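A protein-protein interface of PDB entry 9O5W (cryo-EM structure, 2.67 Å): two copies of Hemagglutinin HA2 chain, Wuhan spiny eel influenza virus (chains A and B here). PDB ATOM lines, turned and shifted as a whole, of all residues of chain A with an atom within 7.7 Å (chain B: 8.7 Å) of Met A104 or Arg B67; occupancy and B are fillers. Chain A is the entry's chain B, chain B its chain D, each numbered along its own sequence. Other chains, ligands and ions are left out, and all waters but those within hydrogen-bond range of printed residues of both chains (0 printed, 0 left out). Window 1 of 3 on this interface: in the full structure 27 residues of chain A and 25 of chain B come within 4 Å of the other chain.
Asp A92 touches Ser B70.
Val A93 touches Arg B94 (CG1 to CD, 3.7 Å).
Asp A96 touches Arg B67 (CB to O, 3.5 Å).
OE2 of Glu A97 touches OG1 of Thr B98 (3.9 Å).
Ala A100 touches Arg B67 (CB to NE, 3.4 Å).
NE2 of Gln B101 touches NE2 of Gln A101, 3.8 Å away.
Leu A107 touches Asn B60.
Of the printed residues of chain B, Met A104 touches Arg B67 (2.8 Å).
Arg B67 touches four residues of chain A.
Of the printed residues of chain B, Asp A96 touches Arg B67 (3.5 Å), Phe B69 (3.2 Å) and Ser B70 (2.5 Å).
Of the printed residues of chain A, Asn B60 touches Leu A107 (3.6 Å).
Val A106 touches none of the printed residues of chain B.
The nearest printed residue of chain A that does not touch Asn B60 is Met A104 (4.7 Å).
OD1 of Asn B60 lies close to NZ of Lys B63.
O of Arg B94 is in hydrogen-bond range of OG1 of Thr B98.
NH2 of Arg B94 sits at hydrogen-bond distance from O of Arg B67 (3.3 Å).
The side-chain amide oxygen (OE1) of Gln B101 lies within hydrogen-bond range of the guanidinium group (NH1) of Arg B67 (3.0 Å).
SD of Met B64 lies close to NH2 of Arg B67, at 3.6 Å.
Glu A97 touches Thr B98, but with the chains exchanged Thr A98 does not touch Glu B97 (10.5 Å).
Gln B101 touches its own counterpart, Gln A101.
8 positions are printed for both chains.
Of the 12 pairs that touch across the chains among the printed residues, 1 has its exchanged pair printed and touching as well.
The side-chain carboxylate (OE1) of Glu A97 lies within salt-bridge range of the guanidinium group (NH2) of Arg B94.
The side-chain carboxylate (OD2) of Asp A96 is in hydrogen-bond range of the backbone NH (N) of Phe B69 (3.2 Å).
The side-chain carboxylate of Glu A97 lies within salt-bridge range of the guanidinium group of Arg B67 (3.4 Å).
OG of Ser B70 lies within hydrogen-bond range of OD2 of Asp A96, 2.5 Å away.
SD of Met A104 sits at hydrogen-bond distance from NH2 of Arg B67, at 2.8 Å.
Of the 18 printed residues of chain B, 7 touch a printed residue of chain A.
Printed residues of chain B that touch a printed residue of chain A: Asn B60, Arg B67, Phe B69, Ser B70, Arg B94, Thr B98 and Gln B101.
Hydrophobic or aromatic side chains of chain B that line the printed part of chain A: Phe B69.
Printed residues of chain A that touch a printed residue of chain B: Asp A92, Val A93, Asp A96, Glu A97, Ala A100, Gln A101, Met A104 and Leu A107.
Hydrophobic or aromatic side chains of chain A within 4 Å of the printed part of chain B: Val A93, Ala A100, Met A104 and Leu A107.
Among the printed residues, Asp or Glu carboxylates within 4 Å of a Lys or Arg side-chain nitrogen of the other chain: Glu A97 with Arg B67 and Glu A97 with Arg B94.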
ATOM      1  N   MET A  61     -14.114   1.659 -23.737  1.00  0.00           N
ATOM      2  CA  MET A  61     -14.115   0.438 -22.960  1.00  0.00           C
ATOM      3  C   MET A  61     -15.276   0.450 -21.979  1.00  0.00           C
ATOM      4  O   MET A  61     -15.754  -0.611 -21.564  1.00  0.00           O
ATOM      5  CB  MET A  61     -12.762   0.265 -22.271  1.00  0.00           C
ATOM      6  CG  MET A  61     -11.744  -0.249 -23.293  1.00  0.00           C
ATOM      7  SD  MET A  61     -10.058  -0.637 -22.812  1.00  0.00           S
ATOM      8  CE  MET A  61     -10.018  -0.133 -21.118  1.00  0.00           C
ATOM      9  N   MET A  64     -18.734  -1.418 -22.909  1.00  0.00           N
ATOM     10  CA  MET A  64     -18.942  -2.858 -22.953  1.00  0.00           C
ATOM     11  C   MET A  64     -19.743  -3.343 -21.757  1.00  0.00           C
ATOM     12  O   MET A  64     -20.018  -4.544 -21.662  1.00  0.00           O
ATOM     13  CB  MET A  64     -17.620  -3.622 -22.999  1.00  0.00           C
ATOM     14  CG  MET A  64     -16.859  -3.484 -24.289  1.00  0.00           C
ATOM     15  SD  MET A  64     -15.913  -4.983 -24.588  1.00  0.00           S
ATOM     16  CE  MET A  64     -14.285  -4.403 -24.187  1.00  0.00           C
ATOM     17  N   ASP A  92     -24.137 -17.375 -17.379  1.00  0.00           N
ATOM     18  CA  ASP A  92     -22.732 -17.685 -17.137  1.00  0.00           C
ATOM     19  C   ASP A  92     -21.903 -17.667 -18.415  1.00  0.00           C
ATOM     20  O   ASP A  92     -20.759 -17.198 -18.399  1.00  0.00           O
ATOM     21  CB  ASP A  92     -22.639 -19.061 -16.475  1.00  0.00           C
ATOM     22  CG  ASP A  92     -23.087 -19.049 -15.023  1.00  0.00           C
ATOM     23  OD1 ASP A  92     -23.277 -17.954 -14.453  1.00  0.00           O
ATOM     24  OD2 ASP A  92     -23.249 -20.145 -14.449  1.00  0.00           O
ATOM     25  N   VAL A  93     -22.475 -18.098 -19.538  1.00  0.00           N
ATOM     26  CA  VAL A  93     -21.743 -18.039 -20.798  1.00  0.00           C
ATOM     27  C   VAL A  93     -21.544 -16.584 -21.190  1.00  0.00           C
ATOM     28  O   VAL A  93     -20.451 -16.180 -21.614  1.00  0.00           O
ATOM     29  CB  VAL A  93     -22.469 -18.854 -21.887  1.00  0.00           C
ATOM     30  CG1 VAL A  93     -21.853 -18.637 -23.276  1.00  0.00           C
ATOM     31  CG2 VAL A  93     -22.402 -20.336 -21.556  1.00  0.00           C
ATOM     32  N   ALA A  95     -21.458 -13.950 -19.252  1.00  0.00           N
ATOM     33  CA  ALA A  95     -20.501 -13.312 -18.355  1.00  0.00           C
ATOM     34  C   ALA A  95     -19.067 -13.743 -18.646  1.00  0.00           C
ATOM     35  O   ALA A  95     -18.151 -12.908 -18.629  1.00  0.00           O
ATOM     36  CB  ALA A  95     -20.862 -13.625 -16.905  1.00  0.00           C
ATOM     37  N   ASP A  96     -18.851 -15.020 -18.978  1.00  0.00           N
ATOM     38  CA  ASP A  96     -17.484 -15.468 -19.234  1.00  0.00           C
ATOM     39  C   ASP A  96     -16.960 -14.905 -20.547  1.00  0.00           C
ATOM     40  O   ASP A  96     -15.799 -14.470 -20.629  1.00  0.00           O
ATOM     41  CB  ASP A  96     -17.426 -16.995 -19.250  1.00  0.00           C
ATOM     42  CG  ASP A  96     -17.592 -17.607 -17.870  1.00  0.00           C
ATOM     43  OD1 ASP A  96     -17.551 -16.863 -16.869  1.00  0.00           O
ATOM     44  OD2 ASP A  96     -17.761 -18.841 -17.788  1.00  0.00           O
ATOM     45  N   GLU A  97     -17.818 -14.830 -21.565  1.00  0.00           N
ATOM     46  CA  GLU A  97     -17.363 -14.301 -22.843  1.00  0.00           C
ATOM     47  C   GLU A  97     -17.103 -12.808 -22.723  1.00  0.00           C
ATOM     48  O   GLU A  97     -16.137 -12.286 -23.299  1.00  0.00           O
ATOM     49  CB  GLU A  97     -18.401 -14.587 -23.928  1.00  0.00           C
ATOM     50  CG  GLU A  97     -18.535 -16.058 -24.305  1.00  0.00           C
ATOM     51  CD  GLU A  97     -17.294 -16.617 -24.973  1.00  0.00           C
ATOM     52  OE1 GLU A  97     -16.447 -17.199 -24.264  1.00  0.00           O
ATOM     53  OE2 GLU A  97     -17.168 -16.478 -26.208  1.00  0.00           O
ATOM     54  N   THR A  98     -17.925 -12.112 -21.935  1.00  0.00           N
ATOM     55  CA  THR A  98     -17.717 -10.686 -21.740  1.00  0.00           C
ATOM     56  C   THR A  98     -16.404 -10.435 -21.007  1.00  0.00           C
ATOM     57  O   THR A  98     -15.648  -9.531 -21.382  1.00  0.00           O
ATOM     58  CB  THR A  98     -18.908 -10.092 -20.981  1.00  0.00           C
ATOM     59  OG1 THR A  98     -20.098 -10.269 -21.757  1.00  0.00           O
ATOM     60  CG2 THR A  98     -18.728  -8.597 -20.715  1.00  0.00           C
ATOM     61  N   ALA A  99     -16.122 -11.204 -19.949  1.00  0.00           N
ATOM     62  CA  ALA A  99     -14.872 -11.001 -19.224  1.00  0.00           C
ATOM     63  C   ALA A  99     -13.665 -11.257 -20.121  1.00  0.00           C
ATOM     64  O   ALA A  99     -12.676 -10.508 -20.078  1.00  0.00           O
ATOM     65  CB  ALA A  99     -14.825 -11.912 -17.997  1.00  0.00           C
ATOM     66  N   ALA A 100     -13.734 -12.296 -20.963  1.00  0.00           N
ATOM     67  CA  ALA A 100     -12.611 -12.582 -21.852  1.00  0.00           C
ATOM     68  C   ALA A 100     -12.406 -11.459 -22.865  1.00  0.00           C
ATOM     69  O   ALA A 100     -11.266 -11.050 -23.139  1.00  0.00           O
ATOM     70  CB  ALA A 100     -12.837 -13.913 -22.565  1.00  0.00           C
ATOM     71  N   GLN A 101     -13.506 -10.912 -23.390  1.00  0.00           N
ATOM     72  CA  GLN A 101     -13.395  -9.823 -24.351  1.00  0.00           C
ATOM     73  C   GLN A 101     -12.831  -8.575 -23.690  1.00  0.00           C
ATOM     74  O   GLN A 101     -12.039  -7.845 -24.300  1.00  0.00           O
ATOM     75  CB  GLN A 101     -14.756  -9.541 -24.981  1.00  0.00           C
ATOM     76  CG  GLN A 101     -15.206 -10.632 -25.933  1.00  0.00           C
ATOM     77  CD  GLN A 101     -16.632 -10.442 -26.403  1.00  0.00           C
ATOM     78  OE1 GLN A 101     -17.155  -9.329 -26.401  1.00  0.00           O
ATOM     79  NE2 GLN A 101     -17.268 -11.532 -26.817  1.00  0.00           N
ATOM     80  N   ILE A 102     -13.210  -8.325 -22.435  1.00  0.00           N
ATOM     81  CA  ILE A 102     -12.699  -7.152 -21.738  1.00  0.00           C
ATOM     82  C   ILE A 102     -11.195  -7.289 -21.549  1.00  0.00           C
ATOM     83  O   ILE A 102     -10.440  -6.333 -21.756  1.00  0.00           O
ATOM     84  CB  ILE A 102     -13.444  -6.976 -20.397  1.00  0.00           C
ATOM     85  CG1 ILE A 102     -14.909  -6.596 -20.645  1.00  0.00           C
ATOM     86  CG2 ILE A 102     -12.776  -5.902 -19.509  1.00  0.00           C
ATOM     87  CD1 ILE A 102     -15.820  -6.765 -19.432  1.00  0.00           C
ATOM     88  N   GLU A 103     -10.739  -8.476 -21.142  1.00  0.00           N
ATOM     89  CA  GLU A 103      -9.309  -8.675 -20.926  1.00  0.00           C
ATOM     90  C   GLU A 103      -8.515  -8.495 -22.218  1.00  0.00           C
ATOM     91  O   GLU A 103      -7.462  -7.830 -22.230  1.00  0.00           O
ATOM     92  CB  GLU A 103      -9.058 -10.062 -20.336  1.00  0.00           C
ATOM     93  CG  GLU A 103      -9.592 -10.236 -18.927  1.00  0.00           C
ATOM     94  CD  GLU A 103      -9.594 -11.680 -18.470  1.00  0.00           C
ATOM     95  OE1 GLU A 103      -9.072 -12.543 -19.208  1.00  0.00           O
ATOM     96  OE2 GLU A 103     -10.120 -11.952 -17.372  1.00  0.00           O
ATOM     97  N   MET A 104      -9.048  -8.996 -23.340  1.00  0.00           N
ATOM     98  CA  MET A 104      -8.315  -8.818 -24.590  1.00  0.00           C
ATOM     99  C   MET A 104      -8.331  -7.374 -25.059  1.00  0.00           C
ATOM    100  O   MET A 104      -7.332  -6.890 -25.613  1.00  0.00           O
ATOM    101  CB  MET A 104      -8.937  -9.659 -25.700  1.00  0.00           C
ATOM    102  CG  MET A 104      -8.776 -11.163 -25.585  1.00  0.00           C
ATOM    103  SD  MET A 104     -10.038 -12.177 -26.423  1.00  0.00           S
ATOM    104  CE  MET A 104     -10.843 -11.056 -27.589  1.00  0.00           C
ATOM    105  N   ILE A 105      -9.414  -6.648 -24.794  1.00  0.00           N
ATOM    106  CA  ILE A 105      -9.454  -5.260 -25.224  1.00  0.00           C
ATOM    107  C   ILE A 105      -8.499  -4.427 -24.385  1.00  0.00           C
ATOM    108  O   ILE A 105      -7.876  -3.490 -24.886  1.00  0.00           O
ATOM    109  CB  ILE A 105     -10.902  -4.728 -25.204  1.00  0.00           C
ATOM    110  CG1 ILE A 105     -11.530  -4.779 -26.604  1.00  0.00           C
ATOM    111  CG2 ILE A 105     -10.992  -3.307 -24.676  1.00  0.00           C
ATOM    112  CD1 ILE A 105     -11.482  -6.143 -27.307  1.00  0.00           C
ATOM    113  N   VAL A 106      -8.376  -4.743 -23.094  1.00  0.00           N
ATOM    114  CA  VAL A 106      -7.434  -4.006 -22.258  1.00  0.00           C
ATOM    115  C   VAL A 106      -6.012  -4.231 -22.754  1.00  0.00           C
ATOM    116  O   VAL A 106      -5.215  -3.286 -22.840  1.00  0.00           O
ATOM    117  CB  VAL A 106      -7.615  -4.387 -20.775  1.00  0.00           C
ATOM    118  CG1 VAL A 106      -6.487  -3.834 -19.888  1.00  0.00           C
ATOM    119  CG2 VAL A 106      -8.937  -3.843 -20.267  1.00  0.00           C
ATOM    120  N   LEU A 107      -5.673  -5.477 -23.104  1.00  0.00           N
ATOM    121  CA  LEU A 107      -4.319  -5.726 -23.594  1.00  0.00           C
ATOM    122  C   LEU A 107      -4.062  -4.991 -24.908  1.00  0.00           C
ATOM    123  O   LEU A 107      -2.999  -4.372 -25.096  1.00  0.00           O
ATOM    124  CB  LEU A 107      -4.105  -7.226 -23.797  1.00  0.00           C
ATOM    125  CG  LEU A 107      -4.113  -8.156 -22.586  1.00  0.00           C
ATOM    126  CD1 LEU A 107      -3.979  -9.594 -23.049  1.00  0.00           C
ATOM    127  CD2 LEU A 107      -3.021  -7.812 -21.602  1.00  0.00           C
ATOM    128  N   LEU A 108      -5.063  -4.967 -25.791  1.00  0.00           N
ATOM    129  CA  LEU A 108      -4.885  -4.307 -27.079  1.00  0.00           C
ATOM    130  C   LEU A 108      -4.776  -2.796 -26.916  1.00  0.00           C
ATOM    131  O   LEU A 108      -3.960  -2.149 -27.588  1.00  0.00           O
ATOM    132  CB  LEU A 108      -6.041  -4.679 -28.007  1.00  0.00           C
ATOM    133  CG  LEU A 108      -6.022  -4.157 -29.443  1.00  0.00           C
ATOM    134  CD1 LEU A 108      -4.776  -4.610 -30.193  1.00  0.00           C
ATOM    135  CD2 LEU A 108      -7.272  -4.617 -30.164  1.00  0.00           C
ATOM    136  N   GLU A 109      -5.577  -2.214 -26.023  1.00  0.00           N
ATOM    137  CA  GLU A 109      -5.510  -0.776 -25.812  1.00  0.00           C
ATOM    138  C   GLU A 109      -4.192  -0.386 -25.164  1.00  0.00           C
ATOM    139  O   GLU A 109      -3.650   0.680 -25.468  1.00  0.00           O
ATOM    140  CB  GLU A 109      -6.695  -0.288 -24.968  1.00  0.00           C
ATOM    141  CG  GLU A 109      -8.097  -0.338 -25.626  1.00  0.00           C
ATOM    142  CD  GLU A 109      -8.112  -0.040 -27.118  1.00  0.00           C
ATOM    143  OE1 GLU A 109      -7.518   0.978 -27.528  1.00  0.00           O
ATOM    144  OE2 GLU A 109      -8.712  -0.828 -27.878  1.00  0.00           O
ATOM    145  N   ASN A 110      -3.649  -1.222 -24.275  1.00  0.00           N
ATOM    146  CA  ASN A 110      -2.356  -0.869 -23.698  1.00  0.00           C
ATOM    147  C   ASN A 110      -1.274  -0.894 -24.764  1.00  0.00           C
ATOM    148  O   ASN A 110      -0.396  -0.016 -24.796  1.00  0.00           O
ATOM    149  CB  ASN A 110      -1.996  -1.833 -22.568  1.00  0.00           C
ATOM    150  CG  ASN A 110      -2.780  -1.572 -21.311  1.00  0.00           C
ATOM    151  OD1 ASN A 110      -3.265  -0.468 -21.095  1.00  0.00           O
ATOM    152  ND2 ASN A 110      -2.909  -2.588 -20.470  1.00  0.00           N
ATOM    153  N   ASN B  60      -1.338 -15.147 -27.598  1.00  0.00           N
ATOM    154  CA  ASN B  60      -2.546 -14.445 -27.190  1.00  0.00           C
ATOM    155  C   ASN B  60      -3.770 -14.998 -27.902  1.00  0.00           C
ATOM    156  O   ASN B  60      -4.894 -14.591 -27.594  1.00  0.00           O
ATOM    157  CB  ASN B  60      -2.446 -12.948 -27.474  1.00  0.00           C
ATOM    158  CG  ASN B  60      -3.156 -12.120 -26.426  1.00  0.00           C
ATOM    159  OD1 ASN B  60      -2.750 -12.086 -25.264  1.00  0.00           O
ATOM    160  ND2 ASN B  60      -4.271 -11.513 -26.811  1.00  0.00           N
ATOM    161  N   MET B  61      -3.567 -15.921 -28.840  1.00  0.00           N
ATOM    162  CA  MET B  61      -4.626 -16.608 -29.555  1.00  0.00           C
ATOM    163  C   MET B  61      -4.954 -17.917 -28.852  1.00  0.00           C
ATOM    164  O   MET B  61      -6.069 -18.432 -28.979  1.00  0.00           O
ATOM    165  CB  MET B  61      -4.226 -16.806 -31.015  1.00  0.00           C
ATOM    166  CG  MET B  61      -4.418 -15.490 -31.784  1.00  0.00           C
ATOM    167  SD  MET B  61      -4.142 -15.426 -33.556  1.00  0.00           S
ATOM    168  CE  MET B  61      -3.344 -16.967 -33.881  1.00  0.00           C
ATOM    169  N   ASN B  62      -3.979 -18.449 -28.105  1.00  0.00           N
ATOM    170  CA  ASN B  62      -4.109 -19.674 -27.334  1.00  0.00           C
ATOM    171  C   ASN B  62      -5.000 -19.499 -26.114  1.00  0.00           C
ATOM    172  O   ASN B  62      -5.348 -20.505 -25.489  1.00  0.00           O
ATOM    173  CB  ASN B  62      -2.730 -20.163 -26.862  1.00  0.00           C
ATOM    174  CG  ASN B  62      -1.876 -20.705 -27.988  1.00  0.00           C
ATOM    175  OD1 ASN B  62      -2.095 -21.817 -28.463  1.00  0.00           O
ATOM    176  ND2 ASN B  62      -0.890 -19.925 -28.415  1.00  0.00           N
ATOM    177  N   LYS B  63      -5.383 -18.266 -25.756  1.00  0.00           N
ATOM    178  CA  LYS B  63      -6.240 -18.067 -24.593  1.00  0.00           C
ATOM    179  C   LYS B  63      -7.726 -18.164 -24.906  1.00  0.00           C
ATOM    180  O   LYS B  63      -8.519 -18.229 -23.960  1.00  0.00           O
ATOM    181  CB  LYS B  63      -5.979 -16.724 -23.897  1.00  0.00           C
ATOM    182  CG  LYS B  63      -4.630 -16.614 -23.204  1.00  0.00           C
ATOM    183  CD  LYS B  63      -4.431 -15.230 -22.594  1.00  0.00           C
ATOM    184  CE  LYS B  63      -3.592 -14.318 -23.446  1.00  0.00           C
ATOM    185  NZ  LYS B  63      -2.135 -14.607 -23.323  1.00  0.00           N
ATOM    186  N   MET B  64      -8.143 -18.193 -26.177  1.00  0.00           N
ATOM    187  CA  MET B  64      -9.581 -18.226 -26.431  1.00  0.00           C
ATOM    188  C   MET B  64     -10.139 -19.630 -26.311  1.00  0.00           C
ATOM    189  O   MET B  64     -11.347 -19.813 -26.496  1.00  0.00           O
ATOM    190  CB  MET B  64     -10.026 -17.665 -27.776  1.00  0.00           C
ATOM    191  CG  MET B  64      -9.819 -16.204 -27.960  1.00  0.00           C
ATOM    192  SD  MET B  64     -10.501 -15.826 -29.566  1.00  0.00           S
ATOM    193  CE  MET B  64      -9.045 -15.751 -30.527  1.00  0.00           C
ATOM    194  N   THR B  65      -9.302 -20.616 -25.996  1.00  0.00           N
ATOM    195  CA  THR B  65      -9.766 -21.977 -25.840  1.00  0.00           C
ATOM    196  C   THR B  65      -9.988 -22.274 -24.364  1.00  0.00           C
ATOM    197  O   THR B  65     -10.426 -23.376 -24.018  1.00  0.00           O
ATOM    198  CB  THR B  65      -8.740 -22.969 -26.417  1.00  0.00           C
ATOM    199  OG1 THR B  65      -7.565 -22.970 -25.598  1.00  0.00           O
ATOM    200  CG2 THR B  65      -8.325 -22.596 -27.844  1.00  0.00           C
ATOM    201  N   GLU B  66      -9.691 -21.297 -23.491  1.00  0.00           N
ATOM    202  CA  GLU B  66      -9.776 -21.400 -22.044  1.00  0.00           C
ATOM    203  C   GLU B  66     -10.768 -20.374 -21.495  1.00  0.00           C
ATOM    204  O   GLU B  66     -10.566 -19.852 -20.397  1.00  0.00           O
ATOM    205  CB  GLU B  66      -8.407 -21.230 -21.385  1.00  0.00           C
ATOM    206  CG  GLU B  66      -7.389 -22.285 -21.777  1.00  0.00           C
ATOM    207  CD  GLU B  66      -6.432 -21.814 -22.844  1.00  0.00           C
ATOM    208  OE1 GLU B  66      -6.410 -22.423 -23.932  1.00  0.00           O
ATOM    209  OE2 GLU B  66      -5.693 -20.840 -22.591  1.00  0.00           O
ATOM    210  N   ARG B  67     -11.848 -20.076 -22.227  1.00  0.00           N
ATOM    211  CA  ARG B  67     -12.800 -19.056 -21.791  1.00  0.00           C
ATOM    212  C   ARG B  67     -13.935 -19.619 -20.953  1.00  0.00           C
ATOM    213  O   ARG B  67     -14.866 -18.879 -20.622  1.00  0.00           O
ATOM    214  CB  ARG B  67     -13.402 -18.261 -22.961  1.00  0.00           C
ATOM    215  CG  ARG B  67     -12.454 -17.386 -23.762  1.00  0.00           C
ATOM    216  CD  ARG B  67     -13.275 -16.582 -24.772  1.00  0.00           C
ATOM    217  NE  ARG B  67     -12.498 -15.616 -25.538  1.00  0.00           N
ATOM    218  CZ  ARG B  67     -13.020 -14.736 -26.384  1.00  0.00           C
ATOM    219  NH1 ARG B  67     -14.325 -14.670 -26.604  1.00  0.00           N
ATOM    220  NH2 ARG B  67     -12.219 -13.878 -27.005  1.00  0.00           N
ATOM    221  N   ALA B  68     -13.877 -20.895 -20.587  1.00  0.00           N
ATOM    222  CA  ALA B  68     -14.885 -21.481 -19.720  1.00  0.00           C
ATOM    223  C   ALA B  68     -14.344 -21.317 -18.307  1.00  0.00           C
ATOM    224  O   ALA B  68     -13.313 -21.902 -17.957  1.00  0.00           O
ATOM    225  CB  ALA B  68     -15.143 -22.945 -20.068  1.00  0.00           C
ATOM    226  N   PHE B  69     -15.044 -20.525 -17.504  1.00  0.00           N
ATOM    227  CA  PHE B  69     -14.636 -20.179 -16.148  1.00  0.00           C
ATOM    228  C   PHE B  69     -15.583 -20.737 -15.109  1.00  0.00           C
ATOM    229  O   PHE B  69     -15.146 -21.253 -14.077  1.00  0.00           O
ATOM    230  CB  PHE B  69     -14.633 -18.652 -16.011  1.00  0.00           C
ATOM    231  CG  PHE B  69     -13.819 -17.940 -17.058  1.00  0.00           C
ATOM    232  CD1 PHE B  69     -12.661 -18.492 -17.575  1.00  0.00           C
ATOM    233  CD2 PHE B  69     -14.272 -16.743 -17.584  1.00  0.00           C
ATOM    234  CE1 PHE B  69     -11.943 -17.830 -18.551  1.00  0.00           C
ATOM    235  CE2 PHE B  69     -13.565 -16.084 -18.564  1.00  0.00           C
ATOM    236  CZ  PHE B  69     -12.407 -16.632 -19.059  1.00  0.00           C
ATOM    237  N   SER B  70     -16.874 -20.636 -15.384  1.00  0.00           N
ATOM    238  CA  SER B  70     -17.923 -21.117 -14.510  1.00  0.00           C
ATOM    239  C   SER B  70     -18.312 -22.527 -14.908  1.00  0.00           C
ATOM    240  O   SER B  70     -18.280 -22.886 -16.090  1.00  0.00           O
ATOM    241  CB  SER B  70     -19.147 -20.215 -14.613  1.00  0.00           C
ATOM    242  OG  SER B  70     -19.261 -19.734 -15.940  1.00  0.00           O
ATOM    243  N   ARG B  94     -22.530 -20.650 -28.970  1.00  0.00           N
ATOM    244  CA  ARG B  94     -21.222 -20.326 -28.418  1.00  0.00           C
ATOM    245  C   ARG B  94     -20.110 -20.810 -29.345  1.00  0.00           C
ATOM    246  O   ARG B  94     -19.152 -20.074 -29.614  1.00  0.00           O
ATOM    247  CB  ARG B  94     -21.078 -20.940 -27.026  1.00  0.00           C
ATOM    248  CG  ARG B  94     -19.812 -20.529 -26.292  1.00  0.00           C
ATOM    249  CD  ARG B  94     -19.730 -21.160 -24.918  1.00  0.00           C
ATOM    250  NE  ARG B  94     -18.666 -20.566 -24.118  1.00  0.00           N
ATOM    251  CZ  ARG B  94     -18.360 -20.917 -22.875  1.00  0.00           C
ATOM    252  NH1 ARG B  94     -18.992 -21.902 -22.254  1.00  0.00           N
ATOM    253  NH2 ARG B  94     -17.393 -20.266 -22.238  1.00  0.00           N
ATOM    254  N   GLU B  97     -19.926 -18.578 -32.585  1.00  0.00           N
ATOM    255  CA  GLU B  97     -19.388 -17.243 -32.357  1.00  0.00           C
ATOM    256  C   GLU B  97     -17.899 -17.327 -32.059  1.00  0.00           C
ATOM    257  O   GLU B  97     -17.115 -16.479 -32.512  1.00  0.00           O
ATOM    258  CB  GLU B  97     -20.139 -16.565 -31.210  1.00  0.00           C
ATOM    259  CG  GLU B  97     -21.585 -16.199 -31.529  1.00  0.00           C
ATOM    260  CD  GLU B  97     -21.709 -15.127 -32.594  1.00  0.00           C
ATOM    261  OE1 GLU B  97     -21.863 -15.484 -33.781  1.00  0.00           O
ATOM    262  OE2 GLU B  97     -21.656 -13.930 -32.244  1.00  0.00           O
ATOM    263  N   THR B  98     -17.484 -18.374 -31.344  1.00  0.00           N
ATOM    264  CA  THR B  98     -16.069 -18.547 -31.051  1.00  0.00           C
ATOM    265  C   THR B  98     -15.286 -18.796 -32.334  1.00  0.00           C
ATOM    266  O   THR B  98     -14.204 -18.228 -32.522  1.00  0.00           O
ATOM    267  CB  THR B  98     -15.889 -19.690 -30.048  1.00  0.00           C
ATOM    268  OG1 THR B  98     -16.563 -19.361 -28.828  1.00  0.00           O
ATOM    269  CG2 THR B  98     -14.414 -19.939 -29.726  1.00  0.00           C
ATOM    270  N   ALA B  99     -15.798 -19.660 -33.218  1.00  0.00           N
ATOM    271  CA  ALA B  99     -15.085 -19.925 -34.465  1.00  0.00           C
ATOM    272  C   ALA B  99     -14.954 -18.660 -35.305  1.00  0.00           C
ATOM    273  O   ALA B  99     -13.895 -18.403 -35.897  1.00  0.00           O
ATOM    274  CB  ALA B  99     -15.805 -21.017 -35.255  1.00  0.00           C
ATOM    275  N   GLN B 101     -14.853 -15.556 -34.224  1.00  0.00           N
ATOM    276  CA  GLN B 101     -13.882 -14.669 -33.595  1.00  0.00           C
ATOM    277  C   GLN B 101     -12.463 -15.158 -33.847  1.00  0.00           C
ATOM    278  O   GLN B 101     -11.544 -14.352 -34.036  1.00  0.00           O
ATOM    279  CB  GLN B 101     -14.164 -14.556 -32.099  1.00  0.00           C
ATOM    280  CG  GLN B 101     -15.433 -13.785 -31.781  1.00  0.00           C
ATOM    281  CD  GLN B 101     -15.767 -13.804 -30.305  1.00  0.00           C
ATOM    282  OE1 GLN B 101     -14.898 -14.023 -29.464  1.00  0.00           O
ATOM    283  NE2 GLN B 101     -17.033 -13.566 -29.982  1.00  0.00           N
ATOM    284  N   ILE B 102     -12.265 -16.477 -33.847  1.00  0.00           N
ATOM    285  CA  ILE B 102     -10.934 -17.021 -34.094  1.00  0.00           C
ATOM    286  C   ILE B 102     -10.500 -16.681 -35.517  1.00  0.00           C
ATOM    287  O   ILE B 102      -9.346 -16.305 -35.762  1.00  0.00           O
ATOM    288  CB  ILE B 102     -10.939 -18.539 -33.821  1.00  0.00           C
ATOM    289  CG1 ILE B 102     -11.136 -18.806 -32.323  1.00  0.00           C
ATOM    290  CG2 ILE B 102      -9.625 -19.199 -34.277  1.00  0.00           C
ATOM    291  CD1 ILE B 102     -11.531 -20.240 -31.980  1.00  0.00           C
ATOM    292  N   ILE B 105      -9.461 -13.082 -35.641  1.00  0.00           N
ATOM    293  CA  ILE B 105      -8.202 -12.734 -34.990  1.00  0.00           C
ATOM    294  C   ILE B 105      -7.042 -13.213 -35.843  1.00  0.00           C
ATOM    295  O   ILE B 105      -5.993 -12.573 -35.890  1.00  0.00           O
ATOM    296  CB  ILE B 105      -8.087 -13.259 -33.539  1.00  0.00           C
ATOM    297  CG1 ILE B 105      -6.991 -12.474 -32.794  1.00  0.00           C
ATOM    298  CG2 ILE B 105      -7.733 -14.758 -33.495  1.00  0.00           C
ATOM    299  CD1 ILE B 105      -6.955 -12.644 -31.269  1.00  0.00           C
